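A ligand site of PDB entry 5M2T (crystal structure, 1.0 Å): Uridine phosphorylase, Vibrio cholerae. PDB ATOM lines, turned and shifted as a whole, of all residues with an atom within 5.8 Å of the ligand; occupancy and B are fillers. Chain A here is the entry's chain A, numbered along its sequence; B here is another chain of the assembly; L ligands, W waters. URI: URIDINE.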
ATOM      1  N   GLY A  67      -7.425 -23.432  -1.284  1.00  0.00           N
ATOM      2  CA  GLY A  67      -8.772 -23.935  -1.153  1.00  0.00           C
ATOM      3  C   GLY A  67      -9.682 -22.957  -0.437  1.00  0.00           C
ATOM      4  O   GLY A  67      -9.267 -21.915   0.055  1.00  0.00           O
ATOM      5  N   ILE A  68     -10.937 -23.348  -0.304  1.00  0.00           N
ATOM      6  CA  ILE A  68     -11.941 -22.596   0.454  1.00  0.00           C
ATOM      7  C   ILE A  68     -11.836 -22.976   1.921  1.00  0.00           C
ATOM      8  O   ILE A  68     -11.884 -24.161   2.265  1.00  0.00           O
ATOM      9  CB  ILE A  68     -13.345 -22.887  -0.086  1.00  0.00           C
ATOM     10  CG1 ILE A  68     -13.482 -22.372  -1.511  1.00  0.00           C
ATOM     11  CG2 ILE A  68     -14.414 -22.272   0.837  1.00  0.00           C
ATOM     12  CD1 ILE A  68     -14.745 -22.816  -2.202  1.00  0.00           C
ATOM     13  N   GLY A  69     -11.768 -21.962   2.770  1.00  0.00           N
ATOM     14  CA  GLY A  69     -11.894 -22.115   4.194  1.00  0.00           C
ATOM     15  C   GLY A  69     -10.589 -22.108   4.969  1.00  0.00           C
ATOM     16  O   GLY A  69      -9.495 -22.440   4.468  1.00  0.00           O
ATOM     17  N   ARG A  90      -2.664 -12.680   0.908  1.00  0.00           N
ATOM     18  CA  ARG A  90      -3.889 -13.273   0.390  1.00  0.00           C
ATOM     19  C   ARG A  90      -4.568 -12.311  -0.536  1.00  0.00           C
ATOM     20  O   ARG A  90      -4.689 -11.124  -0.233  1.00  0.00           O
ATOM     21  CB  ARG A  90      -4.818 -13.597   1.560  1.00  0.00           C
ATOM     22  CG  ARG A  90      -6.225 -13.850   1.261  1.00  0.00           C
ATOM     23  CD  ARG A  90      -6.353 -15.110   0.678  1.00  0.00           C
ATOM     24  NE  ARG A  90      -7.719 -15.680   0.629  1.00  0.00           N
ATOM     25  CZ  ARG A  90      -7.908 -16.929   0.254  1.00  0.00           C
ATOM     26  NH1 ARG A  90      -6.817 -17.680   0.006  1.00  0.00           N
ATOM     27  NH2 ARG A  90      -9.153 -17.420   0.098  1.00  0.00           N
ATOM     28  N   THR A  93     -11.790 -12.825  -3.410  1.00  0.00           N
ATOM     29  CA  THR A  93     -13.001 -12.101  -3.731  1.00  0.00           C
ATOM     30  C   THR A  93     -13.812 -11.900  -2.456  1.00  0.00           C
ATOM     31  O   THR A  93     -13.624 -12.605  -1.470  1.00  0.00           O
ATOM     32  CB  THR A  93     -13.857 -12.841  -4.742  1.00  0.00           C
ATOM     33  OG1 THR A  93     -14.205 -14.085  -4.140  1.00  0.00           O
ATOM     34  CG2 THR A  93     -13.152 -13.030  -6.104  1.00  0.00           C
ATOM     35  N   THR A  94     -14.750 -10.977  -2.511  1.00  0.00           N
ATOM     36  CA  THR A  94     -15.493 -10.640  -1.321  1.00  0.00           C
ATOM     37  C   THR A  94     -16.846 -10.074  -1.673  1.00  0.00           C
ATOM     38  O   THR A  94     -17.083  -9.615  -2.786  1.00  0.00           O
ATOM     39  CB  THR A  94     -14.703  -9.684  -0.416  1.00  0.00           C
ATOM     40  OG1 THR A  94     -15.372  -9.601   0.847  1.00  0.00           O
ATOM     41  CG2 THR A  94     -14.577  -8.294  -0.952  1.00  0.00           C
ATOM     42  N   GLY A  95     -17.772 -10.160  -0.701  1.00  0.00           N
ATOM     43  CA  GLY A  95     -19.118  -9.638  -0.819  1.00  0.00           C
ATOM     44  C   GLY A  95     -19.271  -8.435   0.083  1.00  0.00           C
ATOM     45  O   GLY A  95     -19.141  -8.577   1.313  1.00  0.00           O
ATOM     46  N   ALA A  96     -19.518  -7.252  -0.505  1.00  0.00           N
ATOM     47  CA  ALA A  96     -19.653  -6.132   0.368  1.00  0.00           C
ATOM     48  C   ALA A  96     -21.035  -6.144   0.994  1.00  0.00           C
ATOM     49  O   ALA A  96     -22.025  -6.599   0.400  1.00  0.00           O
ATOM     50  CB  ALA A  96     -19.449  -4.848  -0.413  1.00  0.00           C
ATOM     51  N   THR A 160     -18.792 -20.812   6.838  1.00  0.00           N
ATOM     52  CA  THR A 160     -19.724 -21.248   5.823  1.00  0.00           C
ATOM     53  C   THR A 160     -19.999 -20.118   4.825  1.00  0.00           C
ATOM     54  O   THR A 160     -19.846 -18.924   5.082  1.00  0.00           O
ATOM     55  CB  THR A 160     -21.055 -21.742   6.406  1.00  0.00           C
ATOM     56  OG1 THR A 160     -21.712 -20.692   7.118  1.00  0.00           O
ATOM     57  CG2 THR A 160     -20.883 -22.964   7.267  1.00  0.00           C
ATOM     58  N   PHE A 161     -20.384 -20.558   3.615  1.00  0.00           N
ATOM     59  CA  PHE A 161     -20.824 -19.627   2.575  1.00  0.00           C
ATOM     60  C   PHE A 161     -22.268 -19.215   2.788  1.00  0.00           C
ATOM     61  O   PHE A 161     -22.663 -18.115   2.405  1.00  0.00           O
ATOM     62  CB  PHE A 161     -20.629 -20.297   1.202  1.00  0.00           C
ATOM     63  CG  PHE A 161     -20.882 -19.401   0.043  1.00  0.00           C
ATOM     64  CD1 PHE A 161     -19.891 -18.523  -0.387  1.00  0.00           C
ATOM     65  CD2 PHE A 161     -22.081 -19.420  -0.645  1.00  0.00           C
ATOM     66  CE1 PHE A 161     -20.093 -17.714  -1.495  1.00  0.00           C
ATOM     67  CE2 PHE A 161     -22.287 -18.603  -1.737  1.00  0.00           C
ATOM     68  CZ  PHE A 161     -21.302 -17.747  -2.146  1.00  0.00           C
ATOM     69  N   GLN A 165     -23.183 -16.442   6.465  1.00  0.00           N
ATOM     70  CA  GLN A 165     -23.314 -15.190   5.735  1.00  0.00           C
ATOM     71  C   GLN A 165     -24.773 -14.786   5.626  1.00  0.00           C
ATOM     72  O   GLN A 165     -25.159 -13.930   4.838  1.00  0.00           O
ATOM     73  CB  GLN A 165     -22.613 -15.264   4.365  1.00  0.00           C
ATOM     74  CG  GLN A 165     -21.152 -15.662   4.517  1.00  0.00           C
ATOM     75  CD  GLN A 165     -20.313 -15.589   3.273  1.00  0.00           C
ATOM     76  OE1 GLN A 165     -20.531 -14.774   2.392  1.00  0.00           O
ATOM     77  NE2 GLN A 165     -19.302 -16.443   3.216  1.00  0.00           N
ATOM     78  N   ARG A 167     -27.472 -16.309   4.519  1.00  0.00           N
ATOM     79  CA  ARG A 167     -28.189 -16.596   3.296  1.00  0.00           C
ATOM     80  C   ARG A 167     -29.339 -17.550   3.609  1.00  0.00           C
ATOM     81  O   ARG A 167     -29.143 -18.581   4.266  1.00  0.00           O
ATOM     82  CB  ARG A 167     -27.268 -17.236   2.243  1.00  0.00           C
ATOM     83  CG  ARG A 167     -26.272 -16.252   1.636  1.00  0.00           C
ATOM     84  CD  ARG A 167     -25.446 -16.870   0.495  1.00  0.00           C
ATOM     85  NE  ARG A 167     -24.835 -15.845  -0.351  1.00  0.00           N
ATOM     86  CZ  ARG A 167     -23.606 -15.362  -0.222  1.00  0.00           C
ATOM     87  NH1 ARG A 167     -22.789 -15.877   0.643  1.00  0.00           N
ATOM     88  NH2 ARG A 167     -23.186 -14.366  -0.967  1.00  0.00           N
ATOM     89  N   PHE A 194     -17.984  -9.868   3.701  1.00  0.00           N
ATOM     90  CA  PHE A 194     -17.830 -11.271   4.065  1.00  0.00           C
ATOM     91  C   PHE A 194     -16.767 -11.968   3.205  1.00  0.00           C
ATOM     92  O   PHE A 194     -16.730 -11.783   1.973  1.00  0.00           O
ATOM     93  CB  PHE A 194     -19.144 -12.036   3.844  1.00  0.00           C
ATOM     94  CG  PHE A 194     -20.239 -11.858   4.893  1.00  0.00           C
ATOM     95  CD1 PHE A 194     -20.052 -12.315   6.174  1.00  0.00           C
ATOM     96  CD2 PHE A 194     -21.497 -11.361   4.547  1.00  0.00           C
ATOM     97  CE1 PHE A 194     -21.084 -12.233   7.118  1.00  0.00           C
ATOM     98  CE2 PHE A 194     -22.515 -11.319   5.486  1.00  0.00           C
ATOM     99  CZ  PHE A 194     -22.308 -11.734   6.766  1.00  0.00           C
ATOM    100  N   GLU A 195     -16.034 -12.874   3.821  1.00  0.00           N
ATOM    101  CA  GLU A 195     -15.248 -13.900   3.113  1.00  0.00           C
ATOM    102  C   GLU A 195     -15.077 -15.080   4.077  1.00  0.00           C
ATOM    103  O   GLU A 195     -15.774 -15.145   5.078  1.00  0.00           O
ATOM    104  CB  GLU A 195     -14.013 -13.356   2.421  1.00  0.00           C
ATOM    105  CG  GLU A 195     -13.133 -12.617   3.341  1.00  0.00           C
ATOM    106  CD  GLU A 195     -12.372 -13.506   4.291  1.00  0.00           C
ATOM    107  OE1 GLU A 195     -12.715 -13.563   5.481  1.00  0.00           O
ATOM    108  OE2 GLU A 195     -11.434 -14.239   3.872  1.00  0.00           O
ATOM    109  N   MET A 196     -14.173 -16.030   3.762  1.00  0.00           N
ATOM    110  CA  MET A 196     -14.129 -17.288   4.495  1.00  0.00           C
ATOM    111  C   MET A 196     -12.752 -17.722   4.994  1.00  0.00           C
ATOM    112  O   MET A 196     -12.653 -18.852   5.448  1.00  0.00           O
ATOM    113  CB  MET A 196     -14.753 -18.422   3.655  1.00  0.00           C
ATOM    114  CG  MET A 196     -16.215 -18.228   3.363  1.00  0.00           C
ATOM    115  SD  MET A 196     -16.985 -19.483   2.358  1.00  0.00           S
ATOM    116  CE  MET A 196     -16.784 -20.910   3.441  1.00  0.00           C
ATOM    117  N   GLU A 197     -11.705 -16.937   4.843  1.00  0.00           N
ATOM    118  CA  GLU A 197     -10.353 -17.394   5.172  1.00  0.00           C
ATOM    119  C   GLU A 197      -9.560 -16.457   6.054  1.00  0.00           C
ATOM    120  O   GLU A 197      -8.593 -16.895   6.684  1.00  0.00           O
ATOM    121  CB  GLU A 197      -9.546 -17.648   3.888  1.00  0.00           C
ATOM    122  CG  GLU A 197     -10.110 -18.769   3.023  1.00  0.00           C
ATOM    123  CD  GLU A 197     -11.307 -18.416   2.116  1.00  0.00           C
ATOM    124  OE1 GLU A 197     -11.567 -17.205   1.835  1.00  0.00           O
ATOM    125  OE2 GLU A 197     -12.027 -19.361   1.732  1.00  0.00           O
ATOM    126  N   ILE A 219     -16.956  -8.260  -5.612  1.00  0.00           N
ATOM    127  CA  ILE A 219     -17.644  -8.891  -6.751  1.00  0.00           C
ATOM    128  C   ILE A 219     -19.152  -8.821  -6.629  1.00  0.00           C
ATOM    129  O   ILE A 219     -19.850  -9.047  -7.637  1.00  0.00           O
ATOM    130  CB  ILE A 219     -17.171 -10.362  -6.958  1.00  0.00           C
ATOM    131  CG1 ILE A 219     -17.573 -11.308  -5.825  1.00  0.00           C
ATOM    132  CG2 ILE A 219     -15.700 -10.380  -7.286  1.00  0.00           C
ATOM    133  CD1 ILE A 219     -17.357 -12.785  -6.170  1.00  0.00           C
ATOM    134  N   ILE A 220     -19.668  -8.493  -5.456  1.00  0.00           N
ATOM    135  CA  ILE A 220     -21.090  -8.393  -5.271  1.00  0.00           C
ATOM    136  C   ILE A 220     -21.285  -7.520  -4.068  1.00  0.00           C
ATOM    137  O   ILE A 220     -20.398  -7.395  -3.219  1.00  0.00           O
ATOM    138  CB  ILE A 220     -21.715  -9.806  -5.100  1.00  0.00           C
ATOM    139  CG1 ILE A 220     -23.227  -9.765  -5.283  1.00  0.00           C
ATOM    140  CG2 ILE A 220     -21.362 -10.406  -3.744  1.00  0.00           C
ATOM    141  CD1 ILE A 220     -23.829 -11.144  -5.555  1.00  0.00           C
ATOM    142  N   ARG A 222     -24.296  -7.134  -1.208  1.00  0.00           N
ATOM    143  CA  ARG A 222     -25.483  -7.765  -0.661  1.00  0.00           C
ATOM    144  C   ARG A 222     -26.637  -6.781  -0.532  1.00  0.00           C
ATOM    145  O   ARG A 222     -27.779  -7.233  -0.352  1.00  0.00           O
ATOM    146  CB  ARG A 222     -25.177  -8.405   0.710  1.00  0.00           C
ATOM    147  CG  ARG A 222     -24.214  -9.630   0.693  1.00  0.00           C
ATOM    148  CD  ARG A 222     -24.789 -10.903   0.140  1.00  0.00           C
ATOM    149  NE  ARG A 222     -25.901 -11.386   0.948  1.00  0.00           N
ATOM    150  CZ  ARG A 222     -25.742 -12.160   2.030  1.00  0.00           C
ATOM    151  NH1 ARG A 222     -26.800 -12.538   2.724  1.00  0.00           N
ATOM    152  NH2 ARG A 222     -24.562 -12.514   2.449  1.00  0.00           N
ATOM    153  N   PHE B   6     -23.872 -22.874  -7.677  1.00  0.00           N
ATOM    154  CA  PHE B   6     -22.897 -21.793  -7.718  1.00  0.00           C
ATOM    155  C   PHE B   6     -21.460 -22.298  -7.762  1.00  0.00           C
ATOM    156  O   PHE B   6     -20.661 -21.793  -8.564  1.00  0.00           O
ATOM    157  CB  PHE B   6     -23.128 -20.837  -6.547  1.00  0.00           C
ATOM    158  CG  PHE B   6     -22.331 -19.580  -6.623  1.00  0.00           C
ATOM    159  CD1 PHE B   6     -22.715 -18.521  -7.451  1.00  0.00           C
ATOM    160  CD2 PHE B   6     -21.209 -19.432  -5.855  1.00  0.00           C
ATOM    161  CE1 PHE B   6     -21.934 -17.349  -7.485  1.00  0.00           C
ATOM    162  CE2 PHE B   6     -20.439 -18.293  -5.903  1.00  0.00           C
ATOM    163  CZ  PHE B   6     -20.806 -17.250  -6.707  1.00  0.00           C
ATOM    164  N   HIS B   7     -21.095 -23.250  -6.903  1.00  0.00           N
ATOM    165  CA  HIS B   7     -19.714 -23.722  -6.826  1.00  0.00           C
ATOM    166  C   HIS B   7     -19.474 -24.979  -7.640  1.00  0.00           C
ATOM    167  O   HIS B   7     -18.439 -25.122  -8.285  1.00  0.00           O
ATOM    168  CB  HIS B   7     -19.274 -23.998  -5.390  1.00  0.00           C
ATOM    169  CG  HIS B   7     -19.210 -22.779  -4.544  1.00  0.00           C
ATOM    170  ND1 HIS B   7     -20.297 -22.268  -3.876  1.00  0.00           N
ATOM    171  CD2 HIS B   7     -18.185 -21.939  -4.297  1.00  0.00           C
ATOM    172  CE1 HIS B   7     -19.928 -21.182  -3.213  1.00  0.00           C
ATOM    173  NE2 HIS B   7     -18.651 -20.942  -3.467  1.00  0.00           N
ATOM    174  N   ARG B  47     -12.285 -25.503  -8.705  1.00  0.00           N
ATOM    175  CA  ARG B  47     -11.690 -25.439  -7.376  1.00  0.00           C
ATOM    176  C   ARG B  47     -11.468 -26.873  -6.853  1.00  0.00           C
ATOM    177  O   ARG B  47     -11.025 -27.743  -7.629  1.00  0.00           O
ATOM    178  CB  ARG B  47     -12.547 -24.524  -6.465  1.00  0.00           C
ATOM    179  CG  ARG B  47     -12.540 -23.040  -6.850  1.00  0.00           C
ATOM    180  CD  ARG B  47     -13.480 -22.275  -5.909  1.00  0.00           C
ATOM    181  NE  ARG B  47     -13.467 -20.816  -5.971  1.00  0.00           N
ATOM    182  CZ  ARG B  47     -12.775 -20.007  -5.170  1.00  0.00           C
ATOM    183  NH1 ARG B  47     -11.941 -20.467  -4.262  1.00  0.00           N
ATOM    184  NH2 ARG B  47     -12.915 -18.702  -5.318  1.00  0.00           N
ATOM    185  N   ILE B  75     -20.322 -26.416   1.603  1.00  0.00           N
ATOM    186  CA  ILE B  75     -20.766 -25.916   0.317  1.00  0.00           C
ATOM    187  C   ILE B  75     -21.234 -27.058  -0.575  1.00  0.00           C
ATOM    188  O   ILE B  75     -22.302 -26.999  -1.198  1.00  0.00           O
ATOM    189  CB  ILE B  75     -19.634 -25.108  -0.354  1.00  0.00           C
ATOM    190  CG1 ILE B  75     -19.428 -23.773   0.354  1.00  0.00           C
ATOM    191  CG2 ILE B  75     -19.934 -24.908  -1.829  1.00  0.00           C
ATOM    192  CD1 ILE B  75     -18.173 -23.053  -0.050  1.00  0.00           C
HETATM  193  N1  URI L   1     -16.620 -15.024  -0.855  1.00  0.00           N
HETATM  194  C2  URI L   1     -17.558 -15.255   0.148  1.00  0.00           C
HETATM  195  N3  URI L   1     -18.650 -14.409   0.185  1.00  0.00           N
HETATM  196  C4  URI L   1     -18.918 -13.406  -0.734  1.00  0.00           C
HETATM  197  C5  URI L   1     -17.969 -13.285  -1.788  1.00  0.00           C
HETATM  198  C6  URI L   1     -16.896 -14.049  -1.795  1.00  0.00           C
HETATM  199  O2  URI L   1     -17.424 -16.125   0.913  1.00  0.00           O
HETATM  200  O4  URI L   1     -19.963 -12.734  -0.614  1.00  0.00           O
HETATM  201  C1' URI L   1     -15.469 -15.917  -1.122  1.00  0.00           C
HETATM  202  C2' URI L   1     -14.723 -16.640   0.027  1.00  0.00           C
HETATM  203  C3' URI L   1     -14.633 -18.118  -0.423  1.00  0.00           C
HETATM  204  C4' URI L   1     -15.251 -18.115  -1.787  1.00  0.00           C
HETATM  205  O2' URI L   1     -13.449 -16.086   0.238  1.00  0.00           O
HETATM  206  O3' URI L   1     -13.327 -18.677  -0.465  1.00  0.00           O
HETATM  207  O4' URI L   1     -16.045 -16.927  -1.885  1.00  0.00           O
HETATM  208  C5' URI L   1     -16.148 -19.279  -2.040  1.00  0.00           C
HETATM  209  O5' URI L   1     -16.758 -19.135  -3.312  1.00  0.00           O
HETATM  210  O   HOH W   1     -21.870 -12.482   1.385  1.00  0.00           O
HETATM  211  O   HOH W   2     -15.881 -18.704  -5.743  1.00  0.00           O
HETATM  212  O   HOH W   3     -11.721 -14.770  -1.159  1.00  0.00           O
HETATM  213  O   HOH W   4     -10.582 -19.455  -1.041  1.00  0.00           O
HETATM  214  O   HOH W   5     -17.972 -16.367  -4.318  1.00  0.00           O
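A ring nitrogen (NE2) of His 7 of chain B sits at hydrogen-bond distance from an oxygen (O5') of the ligand (2.6 Å). OE2 of Glu 197 sits at hydrogen-bond distance from O3' of the ligand. A nitrogen (N3) of the ligand lies within hydrogen-bond range of the side-chain amide oxygen (OE1) of Gln 165. An oxygen (O4) of the ligand sits close to the backbone NH (N) of Gly 95, at 3.4 Å.
The side-chain sulfur of Met 196 sits close to the backbone NH of Phe 161 (3.8 Å). OG1 of Thr 94 is in hydrogen-bond range of O of Phe 194. N of Glu 197 lies within hydrogen-bond range of OE2 of Glu 195 (2.9 Å). The guanidinium group (NH2) of Arg 90 lies within salt-bridge range of the side-chain carboxylate (OE1) of Glu 197. OE2 of Glu 197 is in hydrogen-bond range of N of Gly 69 (2.8 Å). The backbone carbonyl oxygen of Thr 94 is in hydrogen-bond range of the backbone NH of Ile 219. The side-chain amide oxygen of Gln 165 is in hydrogen-bond range of the guanidinium group of Arg 167 (3.1 Å). The backbone carbonyl oxygen (O) of Thr 160 lies within hydrogen-bond range of the side-chain amide nitrogen (NE2) of Gln 165, 3.2 Å away.
SD of Met 196 sits close to O2 of the ligand. Merely in contact with the ligand: Ile 68, Thr 93, Thr 94, Phe 161, Arg 167, Phe 194 and Glu 195. Within 4 Å of the ligand: Ile 68, Thr 93, Thr 94, Gly 95, Phe 161, Gln 165, Arg 167, Phe 194, Glu 195, Met 196, Glu 197 and His 7 of chain B. Along chain A the residues within 4 Å of the ligand span positions 68 to 197.
Water W3 lies within hydrogen-bond range of an oxygen (O2') of the ligand (2.6 Å) and the backbone carbonyl oxygen of Thr 93 (2.9 Å). Water W2 bridges O5' of the ligand (2.6 Å) and NH2 of Arg 47 of chain B (3.0 Å). Water W1 lies within hydrogen-bond range of an oxygen (O4) of the ligand, the side-chain amide oxygen (OE1) of Gln 165, the guanidinium group (NH2) of Arg 222 and the guanidinium group (NH2) of Arg 167. Water W4 lies within hydrogen-bond range of the guanidinium group of Arg 90, an oxygen (O3') of the ligand, the backbone carbonyl oxygen of Gly 67 and the side-chain carboxylate of Glu 197.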
